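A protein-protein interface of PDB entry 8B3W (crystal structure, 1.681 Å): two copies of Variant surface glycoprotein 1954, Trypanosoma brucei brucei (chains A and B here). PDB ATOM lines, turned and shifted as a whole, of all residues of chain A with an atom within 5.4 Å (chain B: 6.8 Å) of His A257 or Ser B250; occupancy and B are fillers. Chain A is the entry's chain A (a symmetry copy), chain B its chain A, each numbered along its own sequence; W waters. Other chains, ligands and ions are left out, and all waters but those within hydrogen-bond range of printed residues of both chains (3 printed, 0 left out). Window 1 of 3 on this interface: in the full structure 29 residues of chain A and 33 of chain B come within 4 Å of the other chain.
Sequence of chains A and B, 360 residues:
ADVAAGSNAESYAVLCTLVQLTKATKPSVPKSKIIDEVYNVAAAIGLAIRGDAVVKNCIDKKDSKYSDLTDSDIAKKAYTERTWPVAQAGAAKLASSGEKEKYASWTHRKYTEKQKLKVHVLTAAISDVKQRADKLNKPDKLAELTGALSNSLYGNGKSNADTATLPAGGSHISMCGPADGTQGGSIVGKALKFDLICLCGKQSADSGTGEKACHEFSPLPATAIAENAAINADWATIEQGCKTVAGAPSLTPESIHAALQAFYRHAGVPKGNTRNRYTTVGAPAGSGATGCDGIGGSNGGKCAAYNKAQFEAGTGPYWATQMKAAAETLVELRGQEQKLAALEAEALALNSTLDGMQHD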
ATOM      1  N   THR A 252       7.517   1.130  -7.265  1.00  0.00           N
ATOM      2  CA  THR A 252       8.182   1.979  -8.246  1.00  0.00           C
ATOM      3  C   THR A 252       9.617   2.203  -7.791  1.00  0.00           C
ATOM      4  O   THR A 252       9.910   2.151  -6.593  1.00  0.00           O
ATOM      5  CB  THR A 252       7.496   3.354  -8.416  1.00  0.00           C
ATOM      6  OG1 THR A 252       7.622   4.098  -7.199  1.00  0.00           O
ATOM      7  CG2 THR A 252       6.054   3.200  -8.728  1.00  0.00           C
ATOM      8  N   PRO A 253      10.510   2.538  -8.709  1.00  0.00           N
ATOM      9  CA  PRO A 253      11.877   2.884  -8.290  1.00  0.00           C
ATOM     10  C   PRO A 253      11.881   4.125  -7.427  1.00  0.00           C
ATOM     11  O   PRO A 253      12.643   4.224  -6.456  1.00  0.00           O
ATOM     12  CB  PRO A 253      12.620   3.059  -9.629  1.00  0.00           C
ATOM     13  CG  PRO A 253      11.559   3.299 -10.646  1.00  0.00           C
ATOM     14  CD  PRO A 253      10.324   2.583 -10.174  1.00  0.00           C
ATOM     15  N   GLU A 254      10.986   5.067  -7.736  1.00  0.00           N
ATOM     16  CA  GLU A 254      10.813   6.242  -6.889  1.00  0.00           C
ATOM     17  C   GLU A 254      10.519   5.841  -5.440  1.00  0.00           C
ATOM     18  O   GLU A 254      11.166   6.317  -4.493  1.00  0.00           O
ATOM     19  CB  GLU A 254       9.680   7.109  -7.454  1.00  0.00           C
ATOM     20  CG  GLU A 254       9.932   7.673  -8.883  1.00  0.00           C
ATOM     21  CD  GLU A 254       9.479   6.782 -10.024  1.00  0.00           C
ATOM     22  OE1 GLU A 254       9.626   7.201 -11.201  1.00  0.00           O
ATOM     23  OE2 GLU A 254       9.000   5.673  -9.789  1.00  0.00           O
ATOM     24  N   SER A 255       9.543   4.942  -5.236  1.00  0.00           N
ATOM     25  CA  SER A 255       9.195   4.581  -3.871  1.00  0.00           C
ATOM     26  C   SER A 255      10.367   3.909  -3.158  1.00  0.00           C
ATOM     27  O   SER A 255      10.582   4.131  -1.957  1.00  0.00           O
ATOM     28  CB  SER A 255       7.972   3.662  -3.850  1.00  0.00           C
ATOM     29  OG  SER A 255       6.827   4.319  -4.343  1.00  0.00           O
ATOM     30  N   ILE A 256      11.083   3.023  -3.856  1.00  0.00           N
ATOM     31  CA  ILE A 256      12.126   2.229  -3.210  1.00  0.00           C
ATOM     32  C   ILE A 256      13.244   3.140  -2.713  1.00  0.00           C
ATOM     33  O   ILE A 256      13.650   3.071  -1.548  1.00  0.00           O
ATOM     34  CB  ILE A 256      12.647   1.137  -4.171  1.00  0.00           C
ATOM     35  CG1 ILE A 256      11.593   0.051  -4.373  1.00  0.00           C
ATOM     36  CG2 ILE A 256      13.935   0.495  -3.653  1.00  0.00           C
ATOM     37  CD1 ILE A 256      11.849  -0.902  -5.546  1.00  0.00           C
ATOM     38  N   HIS A 257      13.721   4.051  -3.568  1.00  0.00           N
ATOM     39  CA  HIS A 257      14.832   4.902  -3.155  1.00  0.00           C
ATOM     40  C   HIS A 257      14.379   5.896  -2.097  1.00  0.00           C
ATOM     41  O   HIS A 257      15.153   6.221  -1.184  1.00  0.00           O
ATOM     42  CB  HIS A 257      15.463   5.612  -4.364  1.00  0.00           C
ATOM     43  CG  HIS A 257      16.268   4.703  -5.227  1.00  0.00           C
ATOM     44  ND1 HIS A 257      17.468   4.172  -4.807  1.00  0.00           N
ATOM     45  CD2 HIS A 257      16.052   4.210  -6.474  1.00  0.00           C
ATOM     46  CE1 HIS A 257      17.948   3.378  -5.749  1.00  0.00           C
ATOM     47  NE2 HIS A 257      17.106   3.381  -6.767  1.00  0.00           N
ATOM     48  N   ALA A 258      13.113   6.327  -2.152  1.00  0.00           N
ATOM     49  CA  ALA A 258      12.618   7.198  -1.090  1.00  0.00           C
ATOM     50  C   ALA A 258      12.593   6.449   0.233  1.00  0.00           C
ATOM     51  O   ALA A 258      12.978   6.989   1.273  1.00  0.00           O
ATOM     52  CB  ALA A 258      11.220   7.737  -1.437  1.00  0.00           C
ATOM     53  N   ALA A 259      12.156   5.191   0.211  1.00  0.00           N
ATOM     54  CA  ALA A 259      12.100   4.417   1.451  1.00  0.00           C
ATOM     55  C   ALA A 259      13.509   4.132   1.991  1.00  0.00           C
ATOM     56  O   ALA A 259      13.722   4.145   3.212  1.00  0.00           O
ATOM     57  CB  ALA A 259      11.297   3.129   1.205  1.00  0.00           C
ATOM     58  N   LEU A 260      14.485   3.909   1.105  1.00  0.00           N
ATOM     59  CA  LEU A 260      15.839   3.608   1.579  1.00  0.00           C
ATOM     60  C   LEU A 260      16.506   4.832   2.221  1.00  0.00           C
ATOM     61  O   LEU A 260      17.145   4.713   3.272  1.00  0.00           O
ATOM     62  CB  LEU A 260      16.692   3.077   0.430  1.00  0.00           C
ATOM     63  CG  LEU A 260      16.350   1.668  -0.082  1.00  0.00           C
ATOM     64  CD1 LEU A 260      17.158   1.370  -1.308  1.00  0.00           C
ATOM     65  CD2 LEU A 260      16.601   0.607   0.988  1.00  0.00           C
ATOM     66  N   GLN A 261      16.357   6.015   1.626  1.00  0.00           N
ATOM     67  CA  GLN A 261      16.974   7.202   2.220  1.00  0.00           C
ATOM     68  C   GLN A 261      16.343   7.539   3.566  1.00  0.00           C
ATOM     69  O   GLN A 261      17.046   7.980   4.477  1.00  0.00           O
ATOM     70  CB  GLN A 261      16.903   8.403   1.268  1.00  0.00           C
ATOM     71  CG  GLN A 261      15.531   8.779   0.750  1.00  0.00           C
ATOM     72  CD  GLN A 261      14.879   9.990   1.473  1.00  0.00           C
ATOM     73  OE1 GLN A 261      15.504  11.068   1.639  1.00  0.00           O
ATOM     74  NE2 GLN A 261      13.589   9.823   1.868  1.00  0.00           N
ATOM     75  N   ALA A 262      15.031   7.322   3.722  1.00  0.00           N
ATOM     76  CA  ALA A 262      14.401   7.461   5.034  1.00  0.00           C
ATOM     77  C   ALA A 262      14.984   6.468   6.037  1.00  0.00           C
ATOM     78  O   ALA A 262      15.274   6.820   7.183  1.00  0.00           O
ATOM     79  CB  ALA A 262      12.887   7.263   4.946  1.00  0.00           C
ATOM     80  N   LYS A 324      17.737  -2.143  -4.070  1.00  0.00           N
ATOM     81  CA  LYS A 324      18.273  -1.338  -5.162  1.00  0.00           C
ATOM     82  C   LYS A 324      18.230  -2.102  -6.484  1.00  0.00           C
ATOM     83  O   LYS A 324      17.999  -1.515  -7.547  1.00  0.00           O
ATOM     84  CB  LYS A 324      19.709  -0.892  -4.854  1.00  0.00           C
ATOM     85  CG  LYS A 324      19.838   0.140  -3.706  1.00  0.00           C
ATOM     86  CD  LYS A 324      21.263   0.534  -3.397  1.00  0.00           C
ATOM     87  CE  LYS A 324      21.284   1.639  -2.330  1.00  0.00           C
ATOM     88  NZ  LYS A 324      22.607   1.864  -1.667  1.00  0.00           N
ATOM     89  N   ALA A 327      14.712  -1.898  -7.777  1.00  0.00           N
ATOM     90  CA  ALA A 327      14.526  -0.579  -8.386  1.00  0.00           C
ATOM     91  C   ALA A 327      15.139  -0.530  -9.784  1.00  0.00           C
ATOM     92  O   ALA A 327      14.493  -0.084 -10.744  1.00  0.00           O
ATOM     93  CB  ALA A 327      15.139   0.507  -7.486  1.00  0.00           C
ATOM     94  N   GLN B  20      26.145  12.771   0.730  1.00  0.00           N
ATOM     95  CA  GLN B  20      26.440  11.408   0.290  1.00  0.00           C
ATOM     96  C   GLN B  20      26.039  11.180  -1.161  1.00  0.00           C
ATOM     97  O   GLN B  20      26.658  10.364  -1.861  1.00  0.00           O
ATOM     98  CB  GLN B  20      25.739  10.407   1.204  1.00  0.00           C
ATOM     99  CG  GLN B  20      26.374  10.351   2.591  1.00  0.00           C
ATOM    100  CD  GLN B  20      27.811   9.965   2.523  1.00  0.00           C
ATOM    101  OE1 GLN B  20      28.668  10.779   2.751  1.00  0.00           O
ATOM    102  NE2 GLN B  20      28.081   8.709   2.203  1.00  0.00           N
ATOM    103  N   LEU B  21      25.018  11.902  -1.639  1.00  0.00           N
ATOM    104  CA  LEU B  21      24.639  11.778  -3.041  1.00  0.00           C
ATOM    105  C   LEU B  21      25.768  12.239  -3.954  1.00  0.00           C
ATOM    106  O   LEU B  21      25.938  11.674  -5.048  1.00  0.00           O
ATOM    107  CB  LEU B  21      23.322  12.538  -3.283  1.00  0.00           C
ATOM    108  CG  LEU B  21      22.077  11.740  -2.848  1.00  0.00           C
ATOM    109  CD1 LEU B  21      20.801  12.614  -2.905  1.00  0.00           C
ATOM    110  CD2 LEU B  21      21.841  10.452  -3.645  1.00  0.00           C
ATOM    111  N   ALA B  24      28.314   9.326  -4.394  1.00  0.00           N
ATOM    112  CA  ALA B  24      27.828   8.054  -4.881  1.00  0.00           C
ATOM    113  C   ALA B  24      28.433   7.733  -6.245  1.00  0.00           C
ATOM    114  O   ALA B  24      28.859   8.612  -6.991  1.00  0.00           O
ATOM    115  CB  ALA B  24      26.298   8.103  -4.952  1.00  0.00           C
ATOM    116  N   THR B  25      28.440   6.447  -6.569  1.00  0.00           N
ATOM    117  CA  THR B  25      28.907   5.976  -7.867  1.00  0.00           C
ATOM    118  C   THR B  25      28.082   6.615  -8.989  1.00  0.00           C
ATOM    119  O   THR B  25      26.855   6.611  -8.944  1.00  0.00           O
ATOM    120  CB  THR B  25      28.807   4.451  -7.909  1.00  0.00           C
ATOM    121  OG1 THR B  25      29.585   3.896  -6.843  1.00  0.00           O
ATOM    122  CG2 THR B  25      29.283   3.888  -9.230  1.00  0.00           C
ATOM    123  N   ALA B 248      24.690   5.302   2.300  1.00  0.00           N
ATOM    124  CA  ALA B 248      25.184   5.290   0.921  1.00  0.00           C
ATOM    125  C   ALA B 248      24.015   5.260  -0.066  1.00  0.00           C
ATOM    126  O   ALA B 248      23.817   4.280  -0.792  1.00  0.00           O
ATOM    127  CB  ALA B 248      26.116   4.091   0.714  1.00  0.00           C
ATOM    128  N   PRO B 249      23.202   6.304  -0.108  1.00  0.00           N
ATOM    129  CA  PRO B 249      22.125   6.337  -1.109  1.00  0.00           C
ATOM    130  C   PRO B 249      22.701   6.321  -2.517  1.00  0.00           C
ATOM    131  O   PRO B 249      23.774   6.871  -2.785  1.00  0.00           O
ATOM    132  CB  PRO B 249      21.376   7.648  -0.801  1.00  0.00           C
ATOM    133  CG  PRO B 249      22.385   8.497  -0.039  1.00  0.00           C
ATOM    134  CD  PRO B 249      23.220   7.521   0.736  1.00  0.00           C
ATOM    135  N   SER B 250      21.960   5.689  -3.430  1.00  0.00           N
ATOM    136  CA  SER B 250      22.378   5.644  -4.830  1.00  0.00           C
ATOM    137  C   SER B 250      22.206   6.997  -5.501  1.00  0.00           C
ATOM    138  O   SER B 250      21.264   7.738  -5.205  1.00  0.00           O
ATOM    139  CB  SER B 250      21.557   4.607  -5.591  1.00  0.00           C
ATOM    140  OG  SER B 250      21.765   3.359  -5.004  1.00  0.00           O
ATOM    141  N   LEU B 251      23.082   7.291  -6.470  1.00  0.00           N
ATOM    142  CA  LEU B 251      22.946   8.509  -7.279  1.00  0.00           C
ATOM    143  C   LEU B 251      21.860   8.270  -8.340  1.00  0.00           C
ATOM    144  O   LEU B 251      22.101   7.757  -9.430  1.00  0.00           O
ATOM    145  CB  LEU B 251      24.284   8.908  -7.899  1.00  0.00           C
ATOM    146  CG  LEU B 251      24.269  10.192  -8.712  1.00  0.00           C
ATOM    147  CD1 LEU B 251      23.806  11.362  -7.866  1.00  0.00           C
ATOM    148  CD2 LEU B 251      25.634  10.459  -9.402  1.00  0.00           C
ATOM    149  N   THR B 252      20.644   8.663  -8.012  1.00  0.00           N
ATOM    150  CA  THR B 252      19.496   8.507  -8.897  1.00  0.00           C
ATOM    151  C   THR B 252      18.631   9.756  -8.783  1.00  0.00           C
ATOM    152  O   THR B 252      18.635  10.427  -7.747  1.00  0.00           O
ATOM    153  CB  THR B 252      18.632   7.273  -8.552  1.00  0.00           C
ATOM    154  OG1 THR B 252      18.032   7.460  -7.266  1.00  0.00           O
ATOM    155  CG2 THR B 252      19.452   6.038  -8.515  1.00  0.00           C
ATOM    156  N   PRO B 253      17.820  10.037  -9.790  1.00  0.00           N
ATOM    157  CA  PRO B 253      16.881  11.162  -9.663  1.00  0.00           C
ATOM    158  C   PRO B 253      15.881  10.910  -8.558  1.00  0.00           C
ATOM    159  O   PRO B 253      15.502  11.828  -7.819  1.00  0.00           O
ATOM    160  CB  PRO B 253      16.246  11.249 -11.064  1.00  0.00           C
ATOM    161  CG  PRO B 253      16.476   9.917 -11.690  1.00  0.00           C
ATOM    162  CD  PRO B 253      17.747   9.368 -11.105  1.00  0.00           C
ATOM    163  N   GLU B 254      15.483   9.645  -8.394  1.00  0.00           N
ATOM    164  CA  GLU B 254      14.625   9.270  -7.275  1.00  0.00           C
ATOM    165  C   GLU B 254      15.243   9.694  -5.939  1.00  0.00           C
ATOM    166  O   GLU B 254      14.593  10.342  -5.103  1.00  0.00           O
ATOM    167  CB  GLU B 254      14.388   7.754  -7.309  1.00  0.00           C
ATOM    168  CG  GLU B 254      13.653   7.230  -8.577  1.00  0.00           C
ATOM    169  CD  GLU B 254      14.548   6.860  -9.743  1.00  0.00           C
ATOM    170  OE1 GLU B 254      14.012   6.399 -10.783  1.00  0.00           O
ATOM    171  OE2 GLU B 254      15.764   7.032  -9.667  1.00  0.00           O
ATOM    172  N   SER B 255      16.520   9.348  -5.714  1.00  0.00           N
ATOM    173  CA  SER B 255      17.123   9.682  -4.433  1.00  0.00           C
ATOM    174  C   SER B 255      17.185  11.194  -4.224  1.00  0.00           C
ATOM    175  O   SER B 255      16.991  11.681  -3.101  1.00  0.00           O
ATOM    176  CB  SER B 255      18.525   9.078  -4.322  1.00  0.00           C
ATOM    177  OG  SER B 255      18.482   7.670  -4.335  1.00  0.00           O
ATOM    178  N   ILE B 256      17.537  11.944  -5.273  1.00  0.00           N
ATOM    179  CA  ILE B 256      17.763  13.380  -5.124  1.00  0.00           C
ATOM    180  C   ILE B 256      16.464  14.074  -4.724  1.00  0.00           C
ATOM    181  O   ILE B 256      16.424  14.837  -3.753  1.00  0.00           O
ATOM    182  CB  ILE B 256      18.366  13.970  -6.418  1.00  0.00           C
ATOM    183  CG1 ILE B 256      19.809  13.505  -6.599  1.00  0.00           C
ATOM    184  CG2 ILE B 256      18.329  15.498  -6.415  1.00  0.00           C
ATOM    185  CD1 ILE B 256      20.405  13.741  -7.991  1.00  0.00           C
ATOM    186  N   ALA B 258      13.822  12.748  -3.402  1.00  0.00           N
ATOM    187  CA  ALA B 258      13.407  12.311  -2.073  1.00  0.00           C
ATOM    188  C   ALA B 258      14.181  13.069  -1.006  1.00  0.00           C
ATOM    189  O   ALA B 258      13.613  13.503  -0.001  1.00  0.00           O
ATOM    190  CB  ALA B 258      13.603  10.795  -1.913  1.00  0.00           C
ATOM    191  N   ARG B 334      19.565   8.381 -18.800  1.00  0.00           N
ATOM    192  CA  ARG B 334      18.672   7.257 -19.069  1.00  0.00           C
ATOM    193  C   ARG B 334      18.046   7.390 -20.447  1.00  0.00           C
ATOM    194  O   ARG B 334      17.981   6.422 -21.220  1.00  0.00           O
ATOM    195  CB  ARG B 334      17.561   7.191 -18.025  1.00  0.00           C
ATOM    196  CG  ARG B 334      17.984   6.725 -16.684  1.00  0.00           C
ATOM    197  CD  ARG B 334      16.763   6.608 -15.732  1.00  0.00           C
ATOM    198  NE  ARG B 334      17.197   6.271 -14.382  1.00  0.00           N
ATOM    199  CZ  ARG B 334      16.440   6.380 -13.291  1.00  0.00           C
ATOM    200  NH1 ARG B 334      15.189   6.816 -13.380  1.00  0.00           N
ATOM    201  NH2 ARG B 334      16.942   6.041 -12.111  1.00  0.00           N
HETATM  202  O   HOH W   1      11.700   9.313  -4.929  1.00  0.00           O
HETATM  203  O   HOH W   2      17.936   6.719  -1.585  1.00  0.00           O
HETATM  204  O   HOH W   3      19.205   4.730  -2.411  1.00  0.00           O
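The backbone carbonyl oxygen (O) of Ala B248 is in hydrogen-bond range of the side-chain amino group (NZ) of Lys A324, 2.8 Å away.
The backbone carbonyl oxygen (O) of Ala B258 lies close to the side-chain amide oxygen (OE1) of Gln A261.
O of Ser B250 is in hydrogen-bond range of OG of Ser B255 (2.9 Å).
The side-chain hydroxyl of Thr B252 lies close to the side-chain carboxylate of Glu B254, 3.3 Å away.
The side-chain hydroxyl of Thr B252 sits at hydrogen-bond distance from the backbone NH of Ser B255 (2.9 Å).
The side-chain carboxylate of Glu B254 lies within salt-bridge range of the guanidinium group of Arg B334, at 2.9 Å.
The side-chain carboxylate of Glu A254 sits close to the side-chain hydroxyl of Thr A252, at 3.3 Å.
The side-chain amide nitrogen (NE2) of Gln A261 lies within hydrogen-bond range of the backbone carbonyl oxygen (O) of Ala A258 (3.0 Å).
C of Pro A253 touches CG of Glu B254, 3.8 Å away.
Glu A254 touches Glu B254.
His A257 touches Ser B250.
OG1 of Thr B252 touches CG of His A257 (3.9 Å).
Glu B254 touches His A257 (CB to CB, 3.8 Å).
OG of Ser B255 touches CB of His A257, 3.7 Å away.
CA of Ala A258 touches CB of Ala B258 (3.8 Å).
Lys A324 touches Ser B250.
Of the printed residues of chain B, Glu A254 touches Glu B254.
His A257 touches four residues of chain B.
Ser B250 touches two residues of chain A.
Of the printed residues of chain A, Glu B254 touches Pro A253, Glu A254 and His A257.
The nearest residue of chain B that does not touch His A257 is Ala B258 (4.9 Å).
The nearest printed residue of chain A that does not touch Thr B252 is Pro A253 (6.3 Å).
Of the 15 printed residues of chain B, 6 touch a printed residue of chain A.
Hydrophobic or aromatic side chains of chain A that line the printed part of chain B: Pro A253, His A257 and Ala A258.
Among the printed residues, no Asp or Glu carboxylate lies within 4 Å of a Lys or Arg side-chain nitrogen of the other chain.
Pro A253 touches Glu B254, but with the chains exchanged Glu A254 does not touch Pro B253 (6.8 Å).
Glu A254 touches its own counterpart, Glu B254.
Ala B258 touches its own counterpart, Ala A258.
Water W2 lies within hydrogen-bond range of O of His A257 (2.9 Å) and OG of Ser B255 (3.0 Å).
Water W3 bridges ND1 of His A257 (3.0 Å) and N of Ser B250 (3.1 Å).
Water W1 bridges O of Glu A254 (3.1 Å) and O of Glu B254 (3.1 Å).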
